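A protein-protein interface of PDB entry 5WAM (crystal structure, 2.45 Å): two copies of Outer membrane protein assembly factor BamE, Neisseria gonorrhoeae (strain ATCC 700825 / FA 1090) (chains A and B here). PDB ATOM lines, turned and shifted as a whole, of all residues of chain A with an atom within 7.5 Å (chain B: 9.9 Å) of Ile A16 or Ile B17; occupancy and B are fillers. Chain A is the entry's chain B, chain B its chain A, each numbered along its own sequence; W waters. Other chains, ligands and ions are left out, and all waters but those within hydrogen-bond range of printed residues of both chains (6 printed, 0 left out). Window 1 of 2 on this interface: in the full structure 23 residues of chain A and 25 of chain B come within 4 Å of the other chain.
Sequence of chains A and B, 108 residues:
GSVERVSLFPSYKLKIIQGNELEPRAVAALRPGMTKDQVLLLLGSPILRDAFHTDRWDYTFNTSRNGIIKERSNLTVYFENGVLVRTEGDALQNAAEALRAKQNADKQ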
ATOM      1  N   LYS A  13      10.426   3.902 -25.175  1.00  0.00           N
ATOM      2  CA  LYS A  13      10.871   4.026 -23.794  1.00  0.00           C
ATOM      3  C   LYS A  13      11.533   2.714 -23.398  1.00  0.00           C
ATOM      4  O   LYS A  13      10.922   1.646 -23.521  1.00  0.00           O
ATOM      5  CB  LYS A  13       9.700   4.346 -22.865  1.00  0.00           C
ATOM      6  CG  LYS A  13      10.112   4.612 -21.425  1.00  0.00           C
ATOM      7  CD  LYS A  13       8.911   4.698 -20.494  1.00  0.00           C
ATOM      8  CE  LYS A  13       8.272   3.333 -20.273  1.00  0.00           C
ATOM      9  NZ  LYS A  13       7.174   3.381 -19.266  1.00  0.00           N
ATOM     10  N   LEU A  14      12.778   2.794 -22.937  1.00  0.00           N
ATOM     11  CA  LEU A  14      13.541   1.619 -22.542  1.00  0.00           C
ATOM     12  C   LEU A  14      14.073   1.815 -21.132  1.00  0.00           C
ATOM     13  O   LEU A  14      14.644   2.866 -20.819  1.00  0.00           O
ATOM     14  CB  LEU A  14      14.699   1.361 -23.512  1.00  0.00           C
ATOM     15  CG  LEU A  14      15.601   0.169 -23.186  1.00  0.00           C
ATOM     16  CD1 LEU A  14      14.821  -1.138 -23.247  1.00  0.00           C
ATOM     17  CD2 LEU A  14      16.786   0.135 -24.135  1.00  0.00           C
ATOM     18  N   LYS A  15      13.885   0.808 -20.287  1.00  0.00           N
ATOM     19  CA  LYS A  15      14.409   0.814 -18.929  1.00  0.00           C
ATOM     20  C   LYS A  15      15.667  -0.043 -18.876  1.00  0.00           C
ATOM     21  O   LYS A  15      15.651  -1.200 -19.309  1.00  0.00           O
ATOM     22  CB  LYS A  15      13.366   0.287 -17.942  1.00  0.00           C
ATOM     23  CG  LYS A  15      13.769   0.401 -16.479  1.00  0.00           C
ATOM     24  CD  LYS A  15      12.709  -0.191 -15.566  1.00  0.00           C
ATOM     25  CE  LYS A  15      13.094  -0.054 -14.102  1.00  0.00           C
ATOM     26  NZ  LYS A  15      12.288  -0.957 -13.231  1.00  0.00           N
ATOM     27  N   ILE A  16      16.752   0.526 -18.360  1.00  0.00           N
ATOM     28  CA  ILE A  16      18.003  -0.199 -18.161  1.00  0.00           C
ATOM     29  C   ILE A  16      18.122  -0.517 -16.677  1.00  0.00           C
ATOM     30  O   ILE A  16      18.162   0.393 -15.841  1.00  0.00           O
ATOM     31  CB  ILE A  16      19.213   0.610 -18.653  1.00  0.00           C
ATOM     32  CG1 ILE A  16      19.001   1.078 -20.097  1.00  0.00           C
ATOM     33  CG2 ILE A  16      20.488  -0.220 -18.546  1.00  0.00           C
ATOM     34  CD1 ILE A  16      18.809  -0.046 -21.105  1.00  0.00           C
ATOM     35  N   ILE A  17      18.185  -1.808 -16.351  1.00  0.00           N
ATOM     36  CA  ILE A  17      18.127  -2.239 -14.959  1.00  0.00           C
ATOM     37  C   ILE A  17      19.435  -1.898 -14.259  1.00  0.00           C
ATOM     38  O   ILE A  17      20.528  -2.209 -14.751  1.00  0.00           O
ATOM     39  CB  ILE A  17      17.817  -3.741 -14.873  1.00  0.00           C
ATOM     40  CG1 ILE A  17      16.440  -4.036 -15.479  1.00  0.00           C
ATOM     41  CG2 ILE A  17      17.882  -4.232 -13.427  1.00  0.00           C
ATOM     42  CD1 ILE A  17      15.277  -3.311 -14.801  1.00  0.00           C
ATOM     43  N   GLN A  18      19.320  -1.261 -13.100  1.00  0.00           N
ATOM     44  CA  GLN A  18      20.457  -0.879 -12.279  1.00  0.00           C
ATOM     45  C   GLN A  18      20.779  -1.978 -11.274  1.00  0.00           C
ATOM     46  O   GLN A  18      19.898  -2.723 -10.833  1.00  0.00           O
ATOM     47  CB  GLN A  18      20.154   0.434 -11.551  1.00  0.00           C
ATOM     48  CG  GLN A  18      21.191   0.864 -10.530  1.00  0.00           C
ATOM     49  CD  GLN A  18      20.801   2.147  -9.829  1.00  0.00           C
ATOM     50  OE1 GLN A  18      19.637   2.553  -9.856  1.00  0.00           O
ATOM     51  NE2 GLN A  18      21.772   2.798  -9.198  1.00  0.00           N
ATOM     52  N   GLY A  19      22.056  -2.069 -10.910  1.00  0.00           N
ATOM     53  CA  GLY A  19      22.501  -3.040  -9.930  1.00  0.00           C
ATOM     54  C   GLY A  19      23.791  -3.736 -10.314  1.00  0.00           C
ATOM     55  O   GLY A  19      24.264  -3.604 -11.447  1.00  0.00           O
ATOM     56  N   ASN A  62      27.203  -4.228 -14.079  1.00  0.00           N
ATOM     57  CA  ASN A  62      26.976  -2.960 -14.754  1.00  0.00           C
ATOM     58  C   ASN A  62      28.231  -2.103 -14.671  1.00  0.00           C
ATOM     59  O   ASN A  62      28.910  -2.069 -13.640  1.00  0.00           O
ATOM     60  CB  ASN A  62      25.799  -2.208 -14.132  1.00  0.00           C
ATOM     61  CG  ASN A  62      24.469  -2.583 -14.753  1.00  0.00           C
ATOM     62  OD1 ASN A  62      24.401  -2.980 -15.915  1.00  0.00           O
ATOM     63  ND2 ASN A  62      23.400  -2.445 -13.980  1.00  0.00           N
ATOM     64  N   ILE A  69      24.831   4.152 -17.439  1.00  0.00           N
ATOM     65  CA  ILE A  69      25.213   2.753 -17.588  1.00  0.00           C
ATOM     66  C   ILE A  69      25.653   2.551 -19.031  1.00  0.00           C
ATOM     67  O   ILE A  69      24.861   2.721 -19.963  1.00  0.00           O
ATOM     68  CB  ILE A  69      24.058   1.810 -17.220  1.00  0.00           C
ATOM     69  CG1 ILE A  69      23.656   2.008 -15.757  1.00  0.00           C
ATOM     70  CG2 ILE A  69      24.464   0.354 -17.456  1.00  0.00           C
ATOM     71  CD1 ILE A  69      22.406   1.245 -15.347  1.00  0.00           C
ATOM     72  N   LYS A  70      26.921   2.191 -19.218  1.00  0.00           N
ATOM     73  CA  LYS A  70      27.515   2.131 -20.546  1.00  0.00           C
ATOM     74  C   LYS A  70      27.669   0.718 -21.076  1.00  0.00           C
ATOM     75  O   LYS A  70      27.685   0.528 -22.295  1.00  0.00           O
ATOM     76  CB  LYS A  70      28.894   2.803 -20.536  1.00  0.00           C
ATOM     77  CG  LYS A  70      28.899   4.235 -20.019  1.00  0.00           C
ATOM     78  CD  LYS A  70      28.120   5.185 -20.923  1.00  0.00           C
ATOM     79  CE  LYS A  70      28.834   5.424 -22.243  1.00  0.00           C
ATOM     80  NZ  LYS A  70      28.147   6.462 -23.062  1.00  0.00           N
ATOM     81  N   GLU A  71      27.776  -0.278 -20.200  1.00  0.00           N
ATOM     82  CA  GLU A  71      28.136  -1.614 -20.644  1.00  0.00           C
ATOM     83  C   GLU A  71      27.768  -2.631 -19.574  1.00  0.00           C
ATOM     84  O   GLU A  71      27.893  -2.357 -18.378  1.00  0.00           O
ATOM     85  CB  GLU A  71      29.636  -1.691 -20.953  1.00  0.00           C
ATOM     86  CG  GLU A  71      30.092  -3.029 -21.506  1.00  0.00           C
ATOM     87  CD  GLU A  71      31.553  -3.027 -21.907  1.00  0.00           C
ATOM     88  OE1 GLU A  71      32.287  -2.105 -21.492  1.00  0.00           O
ATOM     89  OE2 GLU A  71      31.963  -3.947 -22.642  1.00  0.00           O
ATOM     90  N   ARG A  72      27.309  -3.797 -20.020  1.00  0.00           N
ATOM     91  CA  ARG A  72      27.141  -4.964 -19.165  1.00  0.00           C
ATOM     92  C   ARG A  72      28.357  -5.862 -19.355  1.00  0.00           C
ATOM     93  O   ARG A  72      28.591  -6.367 -20.458  1.00  0.00           O
ATOM     94  CB  ARG A  72      25.853  -5.716 -19.500  1.00  0.00           C
ATOM     95  CG  ARG A  72      24.660  -5.339 -18.633  1.00  0.00           C
ATOM     96  CD  ARG A  72      24.261  -3.883 -18.795  1.00  0.00           C
ATOM     97  NE  ARG A  72      23.082  -3.562 -17.993  1.00  0.00           N
ATOM     98  CZ  ARG A  72      21.825  -3.721 -18.396  1.00  0.00           C
ATOM     99  NH1 ARG A  72      21.556  -4.198 -19.604  1.00  0.00           N
ATOM    100  NH2 ARG A  72      20.826  -3.404 -17.585  1.00  0.00           N
ATOM    101  N   LEU B  14      14.656   7.857 -28.226  1.00  0.00           N
ATOM    102  CA  LEU B  14      14.774   6.852 -27.179  1.00  0.00           C
ATOM    103  C   LEU B  14      14.876   7.553 -25.835  1.00  0.00           C
ATOM    104  O   LEU B  14      15.805   8.333 -25.608  1.00  0.00           O
ATOM    105  CB  LEU B  14      15.998   5.966 -27.427  1.00  0.00           C
ATOM    106  CG  LEU B  14      16.061   4.597 -26.755  1.00  0.00           C
ATOM    107  CD1 LEU B  14      14.877   3.732 -27.151  1.00  0.00           C
ATOM    108  CD2 LEU B  14      17.365   3.914 -27.133  1.00  0.00           C
ATOM    109  N   LYS B  15      13.918   7.285 -24.952  1.00  0.00           N
ATOM    110  CA  LYS B  15      13.968   7.755 -23.574  1.00  0.00           C
ATOM    111  C   LYS B  15      14.407   6.594 -22.693  1.00  0.00           C
ATOM    112  O   LYS B  15      13.772   5.534 -22.697  1.00  0.00           O
ATOM    113  CB  LYS B  15      12.614   8.295 -23.114  1.00  0.00           C
ATOM    114  CG  LYS B  15      12.645   8.901 -21.718  1.00  0.00           C
ATOM    115  CD  LYS B  15      11.252   9.247 -21.225  1.00  0.00           C
ATOM    116  CE  LYS B  15      11.305  10.064 -19.945  1.00  0.00           C
ATOM    117  NZ  LYS B  15      10.421   9.502 -18.887  1.00  0.00           N
ATOM    118  N   ILE B  16      15.487   6.793 -21.944  1.00  0.00           N
ATOM    119  CA  ILE B  16      16.081   5.744 -21.125  1.00  0.00           C
ATOM    120  C   ILE B  16      15.717   5.992 -19.671  1.00  0.00           C
ATOM    121  O   ILE B  16      15.833   7.120 -19.174  1.00  0.00           O
ATOM    122  CB  ILE B  16      17.608   5.689 -21.307  1.00  0.00           C
ATOM    123  CG1 ILE B  16      17.968   5.465 -22.781  1.00  0.00           C
ATOM    124  CG2 ILE B  16      18.211   4.591 -20.433  1.00  0.00           C
ATOM    125  CD1 ILE B  16      17.415   4.181 -23.377  1.00  0.00           C
ATOM    126  N   ILE B  17      15.269   4.939 -18.993  1.00  0.00           N
ATOM    127  CA  ILE B  17      15.057   4.944 -17.551  1.00  0.00           C
ATOM    128  C   ILE B  17      16.114   4.044 -16.931  1.00  0.00           C
ATOM    129  O   ILE B  17      16.274   2.890 -17.345  1.00  0.00           O
ATOM    130  CB  ILE B  17      13.641   4.463 -17.177  1.00  0.00           C
ATOM    131  CG1 ILE B  17      12.571   5.341 -17.837  1.00  0.00           C
ATOM    132  CG2 ILE B  17      13.467   4.437 -15.659  1.00  0.00           C
ATOM    133  CD1 ILE B  17      12.544   6.781 -17.350  1.00  0.00           C
ATOM    134  N   GLN B  18      16.838   4.570 -15.950  1.00  0.00           N
ATOM    135  CA  GLN B  18      17.854   3.810 -15.230  1.00  0.00           C
ATOM    136  C   GLN B  18      17.377   3.626 -13.794  1.00  0.00           C
ATOM    137  O   GLN B  18      17.266   4.596 -13.038  1.00  0.00           O
ATOM    138  CB  GLN B  18      19.207   4.511 -15.291  1.00  0.00           C
ATOM    139  CG  GLN B  18      19.737   4.669 -16.708  1.00  0.00           C
ATOM    140  CD  GLN B  18      21.168   5.163 -16.754  1.00  0.00           C
ATOM    141  OE1 GLN B  18      22.042   4.521 -17.334  1.00  0.00           O
ATOM    142  NE2 GLN B  18      21.413   6.317 -16.149  1.00  0.00           N
ATOM    143  N   GLY B  19      17.086   2.384 -13.434  1.00  0.00           N
ATOM    144  CA  GLY B  19      16.607   2.072 -12.101  1.00  0.00           C
ATOM    145  C   GLY B  19      16.270   0.602 -12.010  1.00  0.00           C
ATOM    146  O   GLY B  19      16.420  -0.157 -12.975  1.00  0.00           O
ATOM    147  N   ASN B  20      15.813   0.203 -10.823  1.00  0.00           N
ATOM    148  CA  ASN B  20      15.386  -1.172 -10.594  1.00  0.00           C
ATOM    149  C   ASN B  20      14.146  -1.220  -9.713  1.00  0.00           C
ATOM    150  O   ASN B  20      13.944  -2.187  -8.973  1.00  0.00           O
ATOM    151  CB  ASN B  20      16.509  -2.004  -9.970  1.00  0.00           C
ATOM    152  CG  ASN B  20      17.077  -1.372  -8.715  1.00  0.00           C
ATOM    153  OD1 ASN B  20      16.470  -0.479  -8.126  1.00  0.00           O
ATOM    154  ND2 ASN B  20      18.251  -1.834  -8.301  1.00  0.00           N
ATOM    155  N   GLU B  21      13.308  -0.192  -9.784  1.00  0.00           N
ATOM    156  CA  GLU B  21      12.085  -0.170  -8.996  1.00  0.00           C
ATOM    157  C   GLU B  21      11.063  -1.129  -9.590  1.00  0.00           C
ATOM    158  O   GLU B  21      10.939  -1.251 -10.811  1.00  0.00           O
ATOM    159  CB  GLU B  21      11.507   1.243  -8.947  1.00  0.00           C
ATOM    160  CG  GLU B  21      10.389   1.425  -7.934  1.00  0.00           C
ATOM    161  CD  GLU B  21      10.883   1.359  -6.500  1.00  0.00           C
ATOM    162  OE1 GLU B  21      12.113   1.296  -6.295  1.00  0.00           O
ATOM    163  OE2 GLU B  21      10.040   1.373  -5.578  1.00  0.00           O
ATOM    164  N   LEU B  22      10.326  -1.811  -8.719  1.00  0.00           N
ATOM    165  CA  LEU B  22       9.298  -2.732  -9.178  1.00  0.00           C
ATOM    166  C   LEU B  22       8.170  -1.960  -9.848  1.00  0.00           C
ATOM    167  O   LEU B  22       7.663  -0.978  -9.296  1.00  0.00           O
ATOM    168  CB  LEU B  22       8.757  -3.555  -8.010  1.00  0.00           C
ATOM    169  CG  LEU B  22       7.691  -4.596  -8.361  1.00  0.00           C
ATOM    170  CD1 LEU B  22       8.262  -5.677  -9.270  1.00  0.00           C
ATOM    171  CD2 LEU B  22       7.108  -5.211  -7.098  1.00  0.00           C
ATOM    172  N   GLU B  23       7.786  -2.401 -11.047  1.00  0.00           N
ATOM    173  CA  GLU B  23       6.687  -1.812 -11.805  1.00  0.00           C
ATOM    174  C   GLU B  23       5.532  -2.806 -11.809  1.00  0.00           C
ATOM    175  O   GLU B  23       5.452  -3.666 -12.697  1.00  0.00           O
ATOM    176  CB  GLU B  23       7.127  -1.478 -13.233  1.00  0.00           C
ATOM    177  CG  GLU B  23       8.235  -0.433 -13.310  1.00  0.00           C
ATOM    178  CD  GLU B  23       8.684  -0.158 -14.735  1.00  0.00           C
ATOM    179  OE1 GLU B  23       8.786  -1.118 -15.531  1.00  0.00           O
ATOM    180  OE2 GLU B  23       8.932   1.021 -15.063  1.00  0.00           O
ATOM    181  N   LEU B  40      11.550  -7.115 -23.134  1.00  0.00           N
ATOM    182  CA  LEU B  40      12.525  -6.058 -22.877  1.00  0.00           C
ATOM    183  C   LEU B  40      11.845  -4.702 -22.713  1.00  0.00           C
ATOM    184  O   LEU B  40      12.187  -3.932 -21.810  1.00  0.00           O
ATOM    185  CB  LEU B  40      13.554  -6.004 -24.008  1.00  0.00           C
ATOM    186  CG  LEU B  40      14.654  -7.067 -23.993  1.00  0.00           C
ATOM    187  CD1 LEU B  40      15.387  -7.109 -25.328  1.00  0.00           C
ATOM    188  CD2 LEU B  40      15.638  -6.804 -22.863  1.00  0.00           C
ATOM    189  N   LEU B  41      10.886  -4.388 -23.584  1.00  0.00           N
ATOM    190  CA  LEU B  41      10.203  -3.102 -23.503  1.00  0.00           C
ATOM    191  C   LEU B  41       9.254  -3.024 -22.316  1.00  0.00           C
ATOM    192  O   LEU B  41       8.908  -1.919 -21.883  1.00  0.00           O
ATOM    193  CB  LEU B  41       9.434  -2.838 -24.800  1.00  0.00           C
ATOM    194  CG  LEU B  41      10.289  -2.670 -26.056  1.00  0.00           C
ATOM    195  CD1 LEU B  41       9.415  -2.660 -27.299  1.00  0.00           C
ATOM    196  CD2 LEU B  41      11.117  -1.396 -25.976  1.00  0.00           C
ATOM    197  N   LEU B  42       8.830  -4.165 -21.778  1.00  0.00           N
ATOM    198  CA  LEU B  42       7.874  -4.187 -20.681  1.00  0.00           C
ATOM    199  C   LEU B  42       8.566  -4.122 -19.322  1.00  0.00           C
ATOM    200  O   LEU B  42       8.212  -3.288 -18.482  1.00  0.00           O
ATOM    201  CB  LEU B  42       7.009  -5.447 -20.781  1.00  0.00           C
ATOM    202  CG  LEU B  42       5.858  -5.575 -19.782  1.00  0.00           C
ATOM    203  CD1 LEU B  42       4.854  -4.447 -19.955  1.00  0.00           C
ATOM    204  CD2 LEU B  42       5.181  -6.924 -19.949  1.00  0.00           C
ATOM    205  N   LEU B  43       9.553  -4.988 -19.094  1.00  0.00           N
ATOM    206  CA  LEU B  43      10.236  -5.072 -17.811  1.00  0.00           C
ATOM    207  C   LEU B  43      11.547  -4.304 -17.776  1.00  0.00           C
ATOM    208  O   LEU B  43      11.938  -3.815 -16.710  1.00  0.00           O
ATOM    209  CB  LEU B  43      10.520  -6.537 -17.457  1.00  0.00           C
ATOM    210  CG  LEU B  43       9.318  -7.473 -17.351  1.00  0.00           C
ATOM    211  CD1 LEU B  43       9.800  -8.881 -17.048  1.00  0.00           C
ATOM    212  CD2 LEU B  43       8.340  -6.995 -16.285  1.00  0.00           C
ATOM    213  N   GLY B  44      12.229  -4.191 -18.905  1.00  0.00           N
ATOM    214  CA  GLY B  44      13.522  -3.543 -18.976  1.00  0.00           C
ATOM    215  C   GLY B  44      14.614  -4.511 -19.396  1.00  0.00           C
ATOM    216  O   GLY B  44      14.425  -5.724 -19.468  1.00  0.00           O
ATOM    217  N   SER B  45      15.776  -3.933 -19.672  1.00  0.00           N
ATOM    218  CA  SER B  45      16.928  -4.708 -20.113  1.00  0.00           C
ATOM    219  C   SER B  45      17.646  -5.282 -18.898  1.00  0.00           C
ATOM    220  O   SER B  45      18.245  -4.524 -18.125  1.00  0.00           O
ATOM    221  CB  SER B  45      17.879  -3.837 -20.936  1.00  0.00           C
ATOM    222  OG  SER B  45      19.103  -4.510 -21.176  1.00  0.00           O
ATOM    223  N   PRO B  46      17.619  -6.596 -18.690  1.00  0.00           N
ATOM    224  CA  PRO B  46      18.268  -7.164 -17.503  1.00  0.00           C
ATOM    225  C   PRO B  46      19.780  -7.018 -17.583  1.00  0.00           C
ATOM    226  O   PRO B  46      20.356  -6.672 -18.616  1.00  0.00           O
ATOM    227  CB  PRO B  46      17.839  -8.632 -17.532  1.00  0.00           C
ATOM    228  CG  PRO B  46      17.634  -8.918 -18.973  1.00  0.00           C
ATOM    229  CD  PRO B  46      17.088  -7.651 -19.573  1.00  0.00           C
ATOM    230  N   ILE B  47      20.430  -7.291 -16.454  1.00  0.00           N
ATOM    231  CA  ILE B  47      21.880  -7.175 -16.368  1.00  0.00           C
ATOM    232  C   ILE B  47      22.492  -8.394 -17.049  1.00  0.00           C
ATOM    233  O   ILE B  47      22.999  -9.309 -16.390  1.00  0.00           O
ATOM    234  CB  ILE B  47      22.338  -7.023 -14.906  1.00  0.00           C
ATOM    235  CG1 ILE B  47      21.614  -5.829 -14.269  1.00  0.00           C
ATOM    236  CG2 ILE B  47      23.848  -6.828 -14.837  1.00  0.00           C
ATOM    237  CD1 ILE B  47      21.894  -5.620 -12.798  1.00  0.00           C
ATOM    238  N   LEU B  48      22.425  -8.411 -18.379  1.00  0.00           N
ATOM    239  CA  LEU B  48      22.968  -9.477 -19.206  1.00  0.00           C
ATOM    240  C   LEU B  48      23.695  -8.854 -20.384  1.00  0.00           C
ATOM    241  O   LEU B  48      23.197  -7.903 -20.995  1.00  0.00           O
ATOM    242  CB  LEU B  48      21.869 -10.414 -19.729  1.00  0.00           C
ATOM    243  CG  LEU B  48      21.389 -11.552 -18.833  1.00  0.00           C
ATOM    244  CD1 LEU B  48      20.187 -12.226 -19.479  1.00  0.00           C
ATOM    245  CD2 LEU B  48      22.502 -12.558 -18.591  1.00  0.00           C
ATOM    246  N   TYR B  59      15.947 -10.803 -12.830  1.00  0.00           N
ATOM    247  CA  TYR B  59      15.786  -9.432 -12.377  1.00  0.00           C
ATOM    248  C   TYR B  59      15.810  -9.387 -10.857  1.00  0.00           C
ATOM    249  O   TYR B  59      15.375 -10.325 -10.182  1.00  0.00           O
ATOM    250  CB  TYR B  59      14.465  -8.822 -12.857  1.00  0.00           C
ATOM    251  CG  TYR B  59      14.317  -8.657 -14.352  1.00  0.00           C
ATOM    252  CD1 TYR B  59      13.882  -9.707 -15.148  1.00  0.00           C
ATOM    253  CD2 TYR B  59      14.571  -7.436 -14.962  1.00  0.00           C
ATOM    254  CE1 TYR B  59      13.729  -9.554 -16.510  1.00  0.00           C
ATOM    255  CE2 TYR B  59      14.419  -7.273 -16.325  1.00  0.00           C
ATOM    256  CZ  TYR B  59      13.996  -8.334 -17.094  1.00  0.00           C
ATOM    257  OH  TYR B  59      13.842  -8.177 -18.452  1.00  0.00           O
ATOM    258  N   THR B  60      16.320  -8.280 -10.324  1.00  0.00           N
ATOM    259  CA  THR B  60      16.215  -7.968  -8.902  1.00  0.00           C
ATOM    260  C   THR B  60      15.623  -6.571  -8.790  1.00  0.00           C
ATOM    261  O   THR B  60      16.270  -5.585  -9.160  1.00  0.00           O
ATOM    262  CB  THR B  60      17.573  -8.047  -8.201  1.00  0.00           C
ATOM    263  OG1 THR B  60      18.091  -9.378  -8.303  1.00  0.00           O
ATOM    264  CG2 THR B  60      17.441  -7.673  -6.726  1.00  0.00           C
ATOM    265  N   PHE B  61      14.397  -6.487  -8.289  1.00  0.00           N
ATOM    266  CA  PHE B  61      13.691  -5.224  -8.166  1.00  0.00           C
ATOM    267  C   PHE B  61      13.692  -4.749  -6.719  1.00  0.00           C
ATOM    268  O   PHE B  61      13.837  -5.537  -5.781  1.00  0.00           O
ATOM    269  CB  PHE B  61      12.253  -5.361  -8.671  1.00  0.00           C
ATOM    270  CG  PHE B  61      12.150  -5.714 -10.129  1.00  0.00           C
ATOM    271  CD1 PHE B  61      12.588  -4.831 -11.104  1.00  0.00           C
ATOM    272  CD2 PHE B  61      11.603  -6.923 -10.523  1.00  0.00           C
ATOM    273  CE1 PHE B  61      12.490  -5.153 -12.446  1.00  0.00           C
ATOM    274  CE2 PHE B  61      11.501  -7.250 -11.865  1.00  0.00           C
ATOM    275  CZ  PHE B  61      11.945  -6.362 -12.827  1.00  0.00           C
HETATM  276  O   HOH W   1      11.647  -0.866 -21.158  1.00  0.00           O
HETATM  277  O   HOH W   2      18.936  -4.953  -9.939  1.00  0.00           O
HETATM  278  O   HOH W   3      22.423   3.422 -19.908  1.00  0.00           O
HETATM  279  O   HOH W   4       8.705   0.719 -22.723  1.00  0.00           O
HETATM  280  O   HOH W   5      10.624  -3.039 -14.842  1.00  0.00           O
HETATM  281  O   HOH W   6      23.237  -5.464 -22.057  1.00  0.00           O
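O of Leu A14 touches CA of Ile B16 (3.2 Å). CA of Lys A15 touches O of Ile B17, 3.2 Å away. Gly B19 touches Lys A15 (O to CE, 3.5 Å). Leu B43 touches Lys A15. CG2 of Ile B16 touches CG1 of Ile A16, 3.6 Å away. O of Ile A16 touches CA of Gln B18, at 3.5 Å. Ser B45 touches Ile A16 (CB to CD1, 3.9 Å). CA of Ile A17 touches O of Gly B19 (3.3 Å). CD1 of Ile A17 touches O of Leu B43 (3.9 Å). Asn A62 touches Ile B47 (ND2 to CD1, 3.7 Å).
Leu A14 touches just these residues of chain B: Lys B15 (2.9 Å), Ile B16 (3.2 Å) and Ile B17 (2.8 Å). Of chain B, only Ile B16 (3.6 Å), Ile B17 (2.6 Å), Gln B18 (3.5 Å), Gly B19 (3.3 Å) and Ser B45 (3.9 Å) come within 4 Å of Ile A16. Ile A17 touches just these residues of chain B: Gly B19, Leu B43, Ser B45, Ile B47 and Tyr B59. Printed residues of chain B within 4 Å of Gly A19: Ile B47. Lys A70 touches none of the printed residues of chain B. Ile B17 touches three residues of chain A. Of the printed residues of chain A, Gln B18 touches Ile A16 (3.5 Å) and Ile A69 (2.8 Å). Of the printed residues of chain A, Gly B19 touches Lys A15, Ile A16, Ile A17 and Gln A18. Printed residues of chain A within 4 Å of Glu B23: Lys A15 (3.99 Å). Of the printed residues of chain A, Tyr B59 touches Ile A17. The nearest residue of chain A that does not touch Ile B17 is Lys A13 (4.4 Å). The nearest printed residue of chain B that does not touch Lys A13 is Ile B17 (4.4 Å).
The backbone NH of Leu A14 is in hydrogen-bond range of the backbone carbonyl oxygen of Lys B15, 2.9 Å away. The backbone NH (N) of Ile B17 lies within hydrogen-bond range of the backbone carbonyl oxygen (O) of Leu A14 (2.8 Å). The backbone carbonyl oxygen (O) of Ile B17 is in hydrogen-bond range of the backbone NH (N) of Ile A16 (2.6 Å). N of Ile A69 lies within hydrogen-bond range of OE1 of Gln B18, 2.8 Å away. N of Gly B19 lies within hydrogen-bond range of O of Ile A16 (3.3 Å). The backbone carbonyl oxygen (O) of Gly B19 sits at hydrogen-bond distance from the backbone NH (N) of Gln A18 (3.1 Å). O of Gln A18 is in hydrogen-bond range of ND2 of Asn B20, 3.1 Å away. The backbone carbonyl oxygen of Glu B21 lies within hydrogen-bond range of the side-chain amino group of Lys A15, 2.8 Å away. O of Lys A15 is in hydrogen-bond range of N of Ser B45 (2.8 Å). O of Ser B45 lies close to N of Ile A17 (3.2 Å). The backbone carbonyl oxygen (O) of Ser B45 sits at hydrogen-bond distance from the guanidinium group (NH2) of Arg A72 (2.9 Å). The backbone carbonyl oxygen of Pro B46 lies within hydrogen-bond range of the guanidinium group of Arg A72, at 2.9 Å.
OH of Tyr B59 sits at hydrogen-bond distance from O of Gly B44 (2.7 Å). The backbone carbonyl oxygen (O) of Ile A17 lies within hydrogen-bond range of the side-chain amide nitrogen (ND2) of Asn A62, at 3.0 Å. O of Ile A17 lies within hydrogen-bond range of NH2 of Arg A72 (3.1 Å). The backbone carbonyl oxygen (O) of Gly A19 is in hydrogen-bond range of the side-chain amide nitrogen (ND2) of Asn A62 (2.9 Å). The side-chain amide oxygen (OD1) of Asn A62 lies within hydrogen-bond range of the guanidinium group (NE) of Arg A72.
Water W5 lies within hydrogen-bond range of the backbone carbonyl oxygen (O) of Leu B43, the side-chain carboxylate (OE1) of Glu B23 and the side-chain amino group (NZ) of Lys A15. Water W4 lies within hydrogen-bond range of the backbone carbonyl oxygen (O) of Lys A13 and the backbone carbonyl oxygen (O) of Leu B41. Water W3 bridges O of Ile A69 (2.5 Å) and OE1 of Gln B18 (2.8 Å). Water W2 lies within hydrogen-bond range of the backbone carbonyl oxygen of Gln A18 (2.6 Å) and the backbone carbonyl oxygen of Thr B60 (2.8 Å). Water W6 lies within hydrogen-bond range of the backbone carbonyl oxygen of Leu B48 (2.7 Å) and the guanidinium group of Arg A72 (3.2 Å). Water W1 lies within hydrogen-bond range of the backbone NH of Lys A15 (2.9 Å), the backbone carbonyl oxygen of Leu B41 (3.0 Å) and the backbone carbonyl oxygen of Leu B40 (3.2 Å).
Hydrophobic or aromatic side chains of chain B that line the printed part of chain A: Ile B16, Leu B41, Ile B47 and Tyr B59. Hydrophobic or aromatic side chains of chain A within 4 Å of the printed part of chain B: Leu A14, Ile A16, Ile A17 and Ile A69. Along chain A the printed residues that touch a printed residue of chain B span positions 13 to 72. Among the printed residues, 31 pairs touch across the chains.
Ile A16 touches Ile B17, but with the chains exchanged Ile A17 does not touch Ile B16 (7.6 Å). Ile A16 touches Gln B18, but with the chains exchanged Gln A18 does not touch Ile B16 (9.4 Å). Ile A16 touches Gly B19, but with the chains exchanged Gly A19 does not touch Ile B16 (12.2 Å). Ile A17 touches Gly B19, but with the chains exchanged Gly A19 does not touch Ile B17 (10.0 Å).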
